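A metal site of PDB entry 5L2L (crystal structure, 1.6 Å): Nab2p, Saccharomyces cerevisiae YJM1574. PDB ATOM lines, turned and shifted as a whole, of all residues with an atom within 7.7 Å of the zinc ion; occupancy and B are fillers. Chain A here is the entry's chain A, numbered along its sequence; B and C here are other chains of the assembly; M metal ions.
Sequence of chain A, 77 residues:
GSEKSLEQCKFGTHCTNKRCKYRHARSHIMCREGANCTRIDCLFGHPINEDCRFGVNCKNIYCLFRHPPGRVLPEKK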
ATOM      1  N   ASP A  51      14.559   6.530 -25.111  1.00  0.00           N
ATOM      2  CA  ASP A  51      15.234   7.008 -26.319  1.00  0.00           C
ATOM      3  C   ASP A  51      16.585   7.649 -25.975  1.00  0.00           C
ATOM      4  O   ASP A  51      16.669   8.490 -25.071  1.00  0.00           O
ATOM      5  CB  ASP A  51      14.369   8.029 -27.077  1.00  0.00           C
ATOM      6  CG  ASP A  51      13.140   7.403 -27.710  1.00  0.00           C
ATOM      7  OD1 ASP A  51      13.156   6.200 -28.048  1.00  0.00           O
ATOM      8  OD2 ASP A  51      12.127   8.112 -27.862  1.00  0.00           O
ATOM      9  N   CYS A  52      17.625   7.298 -26.732  1.00  0.00           N
ATOM     10  CA  CYS A  52      18.940   7.917 -26.556  1.00  0.00           C
ATOM     11  C   CYS A  52      18.898   9.401 -26.897  1.00  0.00           C
ATOM     12  O   CYS A  52      18.434   9.782 -27.981  1.00  0.00           O
ATOM     13  CB  CYS A  52      19.975   7.234 -27.428  1.00  0.00           C
ATOM     14  SG  CYS A  52      21.682   7.867 -27.136  1.00  0.00           S
ATOM     15  N   ARG A  53      19.438  10.227 -26.000  1.00  0.00           N
ATOM     16  CA  ARG A  53      19.574  11.668 -26.238  1.00  0.00           C
ATOM     17  C   ARG A  53      20.438  11.994 -27.456  1.00  0.00           C
ATOM     18  O   ARG A  53      20.322  13.108 -28.007  1.00  0.00           O
ATOM     19  CB  ARG A  53      20.205  12.352 -25.015  1.00  0.00           C
ATOM     20  CG  ARG A  53      19.285  12.493 -23.819  1.00  0.00           C
ATOM     21  CD  ARG A  53      20.045  12.910 -22.537  1.00  0.00           C
ATOM     22  NE  ARG A  53      19.175  12.911 -21.371  1.00  0.00           N
ATOM     23  CZ  ARG A  53      19.582  13.134 -20.123  1.00  0.00           C
ATOM     24  NH1 ARG A  53      20.868  13.382 -19.867  1.00  0.00           N
ATOM     25  NH2 ARG A  53      18.704  13.089 -19.119  1.00  0.00           N
ATOM     26  N   PHE A  54      21.317  11.095 -27.860  1.00  0.00           N
ATOM     27  CA  PHE A  54      22.304  11.376 -28.901  1.00  0.00           C
ATOM     28  C   PHE A  54      21.936  10.732 -30.244  1.00  0.00           C
ATOM     29  O   PHE A  54      22.672  10.912 -31.223  1.00  0.00           O
ATOM     30  CB  PHE A  54      23.689  10.952 -28.354  1.00  0.00           C
ATOM     31  CG  PHE A  54      23.930  11.525 -26.974  1.00  0.00           C
ATOM     32  CD1 PHE A  54      24.129  12.898 -26.816  1.00  0.00           C
ATOM     33  CD2 PHE A  54      23.837  10.729 -25.840  1.00  0.00           C
ATOM     34  CE1 PHE A  54      24.286  13.457 -25.538  1.00  0.00           C
ATOM     35  CE2 PHE A  54      23.974  11.270 -24.573  1.00  0.00           C
ATOM     36  CZ  PHE A  54      24.196  12.650 -24.413  1.00  0.00           C
ATOM     37  N   GLY A  55      20.780  10.085 -30.340  1.00  0.00           N
ATOM     38  CA  GLY A  55      20.119   9.803 -31.610  1.00  0.00           C
ATOM     39  C   GLY A  55      20.859   8.876 -32.573  1.00  0.00           C
ATOM     40  O   GLY A  55      21.654   7.997 -32.198  1.00  0.00           O
ATOM     41  N   VAL A  56      20.589   9.077 -33.867  1.00  0.00           N
ATOM     42  CA  VAL A  56      21.159   8.180 -34.870  1.00  0.00           C
ATOM     43  C   VAL A  56      22.683   8.333 -34.956  1.00  0.00           C
ATOM     44  O   VAL A  56      23.370   7.375 -35.349  1.00  0.00           O
ATOM     45  CB  VAL A  56      20.483   8.399 -36.244  1.00  0.00           C
ATOM     46  CG1 VAL A  56      20.837   9.751 -36.848  1.00  0.00           C
ATOM     47  CG2 VAL A  56      20.822   7.276 -37.200  1.00  0.00           C
ATOM     48  N   ASN A  57      23.225   9.482 -34.530  1.00  0.00           N
ATOM     49  CA  ASN A  57      24.653   9.773 -34.588  1.00  0.00           C
ATOM     50  C   ASN A  57      25.407   9.421 -33.310  1.00  0.00           C
ATOM     51  O   ASN A  57      26.586   9.780 -33.179  1.00  0.00           O
ATOM     52  CB  ASN A  57      24.870  11.264 -34.911  1.00  0.00           C
ATOM     53  CG  ASN A  57      24.384  11.644 -36.282  1.00  0.00           C
ATOM     54  OD1 ASN A  57      23.697  12.664 -36.458  1.00  0.00           O
ATOM     55  ND2 ASN A  57      24.714  10.837 -37.266  1.00  0.00           N
ATOM     56  N   CYS A  58      24.761   8.740 -32.357  1.00  0.00           N
ATOM     57  CA  CYS A  58      25.429   8.312 -31.133  1.00  0.00           C
ATOM     58  C   CYS A  58      26.618   7.420 -31.467  1.00  0.00           C
ATOM     59  O   CYS A  58      26.470   6.383 -32.117  1.00  0.00           O
ATOM     60  CB  CYS A  58      24.434   7.558 -30.246  1.00  0.00           C
ATOM     61  SG  CYS A  58      25.152   6.902 -28.654  1.00  0.00           S
ATOM     62  N   LYS A  59      27.808   7.812 -31.000  1.00  0.00           N
ATOM     63  CA  LYS A  59      29.048   7.136 -31.355  1.00  0.00           C
ATOM     64  C   LYS A  59      29.469   6.053 -30.370  1.00  0.00           C
ATOM     65  O   LYS A  59      30.499   5.410 -30.594  1.00  0.00           O
ATOM     66  CB  LYS A  59      30.197   8.153 -31.475  1.00  0.00           C
ATOM     67  CG  LYS A  59      30.001   9.180 -32.582  1.00  0.00           C
ATOM     68  CD  LYS A  59      30.266   8.543 -33.949  1.00  0.00           C
ATOM     69  CE  LYS A  59      30.177   9.552 -35.086  1.00  0.00           C
ATOM     70  NZ  LYS A  59      28.785   9.702 -35.582  1.00  0.00           N
ATOM     71  N   ASN A  60      28.715   5.854 -29.285  1.00  0.00           N
ATOM     72  CA  ASN A  60      29.036   4.869 -28.260  1.00  0.00           C
ATOM     73  C   ASN A  60      28.431   3.496 -28.624  1.00  0.00           C
ATOM     74  O   ASN A  60      27.248   3.253 -28.409  1.00  0.00           O
ATOM     75  CB  ASN A  60      28.511   5.357 -26.913  1.00  0.00           C
ATOM     76  CG  ASN A  60      28.672   4.336 -25.804  1.00  0.00           C
ATOM     77  OD1 ASN A  60      29.403   3.345 -25.939  1.00  0.00           O
ATOM     78  ND2 ASN A  60      27.987   4.591 -24.679  1.00  0.00           N
ATOM     79  N   ILE A  61      29.262   2.577 -29.134  1.00  0.00           N
ATOM     80  CA  ILE A  61      28.700   1.321 -29.621  1.00  0.00           C
ATOM     81  C   ILE A  61      28.171   0.445 -28.484  1.00  0.00           C
ATOM     82  O   ILE A  61      27.417  -0.510 -28.745  1.00  0.00           O
ATOM     83  CB  ILE A  61      29.710   0.520 -30.464  1.00  0.00           C
ATOM     84  CG1 ILE A  61      30.903   0.042 -29.643  1.00  0.00           C
ATOM     85  CG2 ILE A  61      30.174   1.337 -31.667  1.00  0.00           C
ATOM     86  CD1 ILE A  61      31.711  -1.002 -30.374  1.00  0.00           C
ATOM     87  N   TYR A  62      28.532   0.746 -27.235  1.00  0.00           N
ATOM     88  CA  TYR A  62      28.047   0.004 -26.072  1.00  0.00           C
ATOM     89  C   TYR A  62      26.769   0.591 -25.478  1.00  0.00           C
ATOM     90  O   TYR A  62      26.235   0.043 -24.496  1.00  0.00           O
ATOM     91  CB  TYR A  62      29.145  -0.046 -25.014  1.00  0.00           C
ATOM     92  CG  TYR A  62      30.472  -0.614 -25.467  1.00  0.00           C
ATOM     93  CD1 TYR A  62      30.544  -1.704 -26.333  1.00  0.00           C
ATOM     94  CD2 TYR A  62      31.681  -0.063 -25.024  1.00  0.00           C
ATOM     95  CE1 TYR A  62      31.766  -2.235 -26.733  1.00  0.00           C
ATOM     96  CE2 TYR A  62      32.896  -0.582 -25.428  1.00  0.00           C
ATOM     97  CZ  TYR A  62      32.939  -1.678 -26.287  1.00  0.00           C
ATOM     98  OH  TYR A  62      34.161  -2.188 -26.700  1.00  0.00           O
ATOM     99  N   CYS A  63      26.225   1.656 -26.071  1.00  0.00           N
ATOM    100  CA  CYS A  63      25.067   2.366 -25.522  1.00  0.00           C
ATOM    101  C   CYS A  63      23.840   1.454 -25.477  1.00  0.00           C
ATOM    102  O   CYS A  63      23.489   0.831 -26.479  1.00  0.00           O
ATOM    103  CB  CYS A  63      24.775   3.607 -26.377  1.00  0.00           C
ATOM    104  SG  CYS A  63      23.460   4.706 -25.762  1.00  0.00           S
ATOM    105  N   LEU A  64      23.158   1.404 -24.328  1.00  0.00           N
ATOM    106  CA  LEU A  64      22.002   0.528 -24.131  1.00  0.00           C
ATOM    107  C   LEU A  64      20.648   1.214 -24.346  1.00  0.00           C
ATOM    108  O   LEU A  64      19.615   0.543 -24.279  1.00  0.00           O
ATOM    109  CB  LEU A  64      22.040  -0.093 -22.706  1.00  0.00           C
ATOM    110  CG  LEU A  64      23.230  -0.997 -22.394  1.00  0.00           C
ATOM    111  CD1 LEU A  64      23.241  -1.361 -20.924  1.00  0.00           C
ATOM    112  CD2 LEU A  64      23.190  -2.262 -23.242  1.00  0.00           C
ATOM    113  N   PHE A  65      20.623   2.531 -24.608  1.00  0.00           N
ATOM    114  CA  PHE A  65      19.390   3.238 -24.883  1.00  0.00           C
ATOM    115  C   PHE A  65      18.871   2.894 -26.299  1.00  0.00           C
ATOM    116  O   PHE A  65      19.542   2.251 -27.115  1.00  0.00           O
ATOM    117  CB  PHE A  65      19.611   4.749 -24.722  1.00  0.00           C
ATOM    118  CG  PHE A  65      19.861   5.178 -23.280  1.00  0.00           C
ATOM    119  CD1 PHE A  65      18.807   5.520 -22.438  1.00  0.00           C
ATOM    120  CD2 PHE A  65      21.136   5.229 -22.762  1.00  0.00           C
ATOM    121  CE1 PHE A  65      19.030   5.914 -21.124  1.00  0.00           C
ATOM    122  CE2 PHE A  65      21.363   5.613 -21.456  1.00  0.00           C
ATOM    123  CZ  PHE A  65      20.308   5.946 -20.637  1.00  0.00           C
ATOM    124  N   ARG A  66      17.655   3.346 -26.603  1.00  0.00           N
ATOM    125  CA  ARG A  66      17.018   3.040 -27.881  1.00  0.00           C
ATOM    126  C   ARG A  66      17.396   4.062 -28.952  1.00  0.00           C
ATOM    127  O   ARG A  66      17.345   5.272 -28.715  1.00  0.00           O
ATOM    128  CB  ARG A  66      15.491   3.016 -27.669  1.00  0.00           C
ATOM    129  CG  ARG A  66      14.682   2.606 -28.864  1.00  0.00           C
ATOM    130  CD  ARG A  66      13.221   2.334 -28.458  1.00  0.00           C
ATOM    131  NE  ARG A  66      12.690   3.359 -27.545  1.00  0.00           N
ATOM    132  CZ  ARG A  66      12.121   3.127 -26.365  1.00  0.00           C
ATOM    133  NH1 ARG A  66      11.970   1.886 -25.897  1.00  0.00           N
ATOM    134  NH2 ARG A  66      11.671   4.141 -25.636  1.00  0.00           N
ATOM    135  N   HIS A  67      17.794   3.572 -30.140  1.00  0.00           N
ATOM    136  CA  HIS A  67      18.219   4.434 -31.242  1.00  0.00           C
ATOM    137  C   HIS A  67      17.319   4.252 -32.471  1.00  0.00           C
ATOM    138  O   HIS A  67      16.735   3.177 -32.661  1.00  0.00           O
ATOM    139  CB  HIS A  67      19.680   4.158 -31.653  1.00  0.00           C
ATOM    140  CG  HIS A  67      20.653   4.279 -30.528  1.00  0.00           C
ATOM    141  ND1 HIS A  67      20.932   3.233 -29.672  1.00  0.00           N
ATOM    142  CD2 HIS A  67      21.419   5.320 -30.118  1.00  0.00           C
ATOM    143  CE1 HIS A  67      21.819   3.637 -28.778  1.00  0.00           C
ATOM    144  NE2 HIS A  67      22.125   4.898 -29.022  1.00  0.00           N
ATOM    145  N   ARG A  71      21.166   3.670 -37.771  1.00  0.00           N
ATOM    146  CA  ARG A  71      22.432   3.730 -37.052  1.00  0.00           C
ATOM    147  C   ARG A  71      23.179   2.424 -37.270  1.00  0.00           C
ATOM    148  O   ARG A  71      22.643   1.352 -36.974  1.00  0.00           O
ATOM    149  CB  ARG A  71      22.190   3.976 -35.562  1.00  0.00           C
ATOM    150  CG  ARG A  71      23.442   4.046 -34.714  1.00  0.00           C
ATOM    151  CD  ARG A  71      23.061   4.417 -33.289  1.00  0.00           C
ATOM    152  NE  ARG A  71      24.176   4.467 -32.332  1.00  0.00           N
ATOM    153  CZ  ARG A  71      24.484   3.517 -31.455  1.00  0.00           C
ATOM    154  NH1 ARG A  71      23.794   2.394 -31.414  1.00  0.00           N
ATOM    155  NH2 ARG A  71      25.486   3.699 -30.606  1.00  0.00           N
ATOM    156  P     A B   5      21.165  12.360 -16.116  1.00  0.00           P
ATOM    157  OP1   A B   5      20.625  13.479 -16.941  1.00  0.00           O
ATOM    158  OP2   A B   5      20.322  11.139 -15.959  1.00  0.00           O
ATOM    159  O5'   A B   5      22.567  11.997 -16.796  1.00  0.00           O
ATOM    160  C5'   A B   5      23.448  11.028 -16.193  1.00  0.00           C
ATOM    161  C4'   A B   5      24.208  10.242 -17.247  1.00  0.00           C
ATOM    162  O4'   A B   5      23.294   9.333 -17.946  1.00  0.00           O
ATOM    163  C3'   A B   5      24.864  11.076 -18.332  1.00  0.00           C
ATOM    164  O3'   A B   5      26.045  10.421 -18.780  1.00  0.00           O
ATOM    165  C2'   A B   5      23.814  11.078 -19.429  1.00  0.00           C
ATOM    166  O2'   A B   5      24.279  11.380 -20.731  1.00  0.00           O
ATOM    167  C1'   A B   5      23.271   9.656 -19.329  1.00  0.00           C
ATOM    168  N9    A B   5      21.890   9.551 -19.822  1.00  0.00           N
ATOM    169  C8    A B   5      20.732   9.771 -19.121  1.00  0.00           C
ATOM    170  N7    A B   5      19.646   9.671 -19.840  1.00  0.00           N
ATOM    171  C5    A B   5      20.109   9.375 -21.121  1.00  0.00           C
ATOM    172  C6    A B   5      19.452   9.132 -22.346  1.00  0.00           C
ATOM    173  N6    A B   5      18.128   9.173 -22.507  1.00  0.00           N
ATOM    174  N1    A B   5      20.207   8.874 -23.432  1.00  0.00           N
ATOM    175  C2    A B   5      21.540   8.832 -23.287  1.00  0.00           C
ATOM    176  N3    A B   5      22.266   9.015 -22.180  1.00  0.00           N
ATOM    177  C4    A B   5      21.494   9.296 -21.118  1.00  0.00           C
ATOM    178  P     A B   6      27.485  11.111 -18.596  1.00  0.00           P
ATOM    179  OP1   A B   6      28.476  10.092 -19.009  1.00  0.00           O
ATOM    180  OP2   A B   6      27.580  11.749 -17.246  1.00  0.00           O
ATOM    181  O5'   A B   6      27.463  12.251 -19.706  1.00  0.00           O
ATOM    182  C5'   A B   6      28.003  13.546 -19.476  1.00  0.00           C
ATOM    183  C4'   A B   6      27.918  14.374 -20.736  1.00  0.00           C
ATOM    184  O4'   A B   6      28.763  13.827 -21.783  1.00  0.00           O
ATOM    185  C3'   A B   6      26.547  14.442 -21.374  1.00  0.00           C
ATOM    186  O3'   A B   6      25.694  15.342 -20.691  1.00  0.00           O
ATOM    187  C2'   A B   6      26.883  14.829 -22.813  1.00  0.00           C
ATOM    188  O2'   A B   6      27.225  16.214 -22.919  1.00  0.00           O
ATOM    189  C1'   A B   6      28.147  14.004 -23.052  1.00  0.00           C
ATOM    190  N9    A B   6      27.851  12.676 -23.636  1.00  0.00           N
ATOM    191  C8    A B   6      27.653  11.480 -22.991  1.00  0.00           C
ATOM    192  N7    A B   6      27.401  10.462 -23.780  1.00  0.00           N
ATOM    193  C5    A B   6      27.419  11.009 -25.042  1.00  0.00           C
ATOM    194  C6    A B   6      27.206  10.450 -26.304  1.00  0.00           C
ATOM    195  N6    A B   6      26.938   9.160 -26.519  1.00  0.00           N
ATOM    196  N1    A B   6      27.303  11.285 -27.370  1.00  0.00           N
ATOM    197  C2    A B   6      27.586  12.583 -27.158  1.00  0.00           C
ATOM    198  N3    A B   6      27.786  13.218 -26.013  1.00  0.00           N
ATOM    199  C4    A B   6      27.689  12.373 -24.969  1.00  0.00           C
ATOM    200  N   HIS C  28      33.217  10.040 -26.974  1.00  0.00           N
ATOM    201  CA  HIS C  28      33.829   8.746 -27.200  1.00  0.00           C
ATOM    202  C   HIS C  28      34.854   8.759 -28.326  1.00  0.00           C
ATOM    203  O   HIS C  28      35.536   7.747 -28.545  1.00  0.00           O
ATOM    204  CB  HIS C  28      32.737   7.696 -27.471  1.00  0.00           C
ATOM    205  CG  HIS C  28      31.807   7.495 -26.323  1.00  0.00           C
ATOM    206  ND1 HIS C  28      30.750   8.345 -26.050  1.00  0.00           N
ATOM    207  CD2 HIS C  28      31.790   6.566 -25.343  1.00  0.00           C
ATOM    208  CE1 HIS C  28      30.124   7.932 -24.969  1.00  0.00           C
ATOM    209  NE2 HIS C  28      30.736   6.848 -24.520  1.00  0.00           N
HETATM  210 ZN    ZN M   1      23.181   6.106 -27.645  1.00  0.00          ZN
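NH1 of Arg 71 is in hydrogen-bond range of ND1 of His 67.
ND1 of His 67 sits at hydrogen-bond distance from O of Phe 65.
NE of Arg 71 sits at hydrogen-bond distance from O of Cys 58 (3.0 Å).
The side-chain sulfur of Cys 58 lies close to N6 of A 6 of chain B (3.6 Å).
The side-chain sulfur of Cys 58 sits close to the backbone NH of Asn 60, 3.8 Å away.
The backbone NH of Phe 65 lies close to the side-chain sulfur of Cys 63, 3.8 Å away.
SG of Cys 52 lies close to N of Phe 54 (3.3 Å).
O of Arg 66 sits at hydrogen-bond distance from N of Cys 52, at 2.8 Å.
The nearest printed residue that does not touch the zinc ion is Arg 71 (4.5 Å).
The zinc ion is bound by a ring nitrogen (NE2) of His 67, the side-chain sulfur (SG) of Cys 58, the side-chain sulfur (SG) of Cys 63 and the side-chain sulfur (SG) of Cys 52.
The zinc ion has four donor atoms within binding distance.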
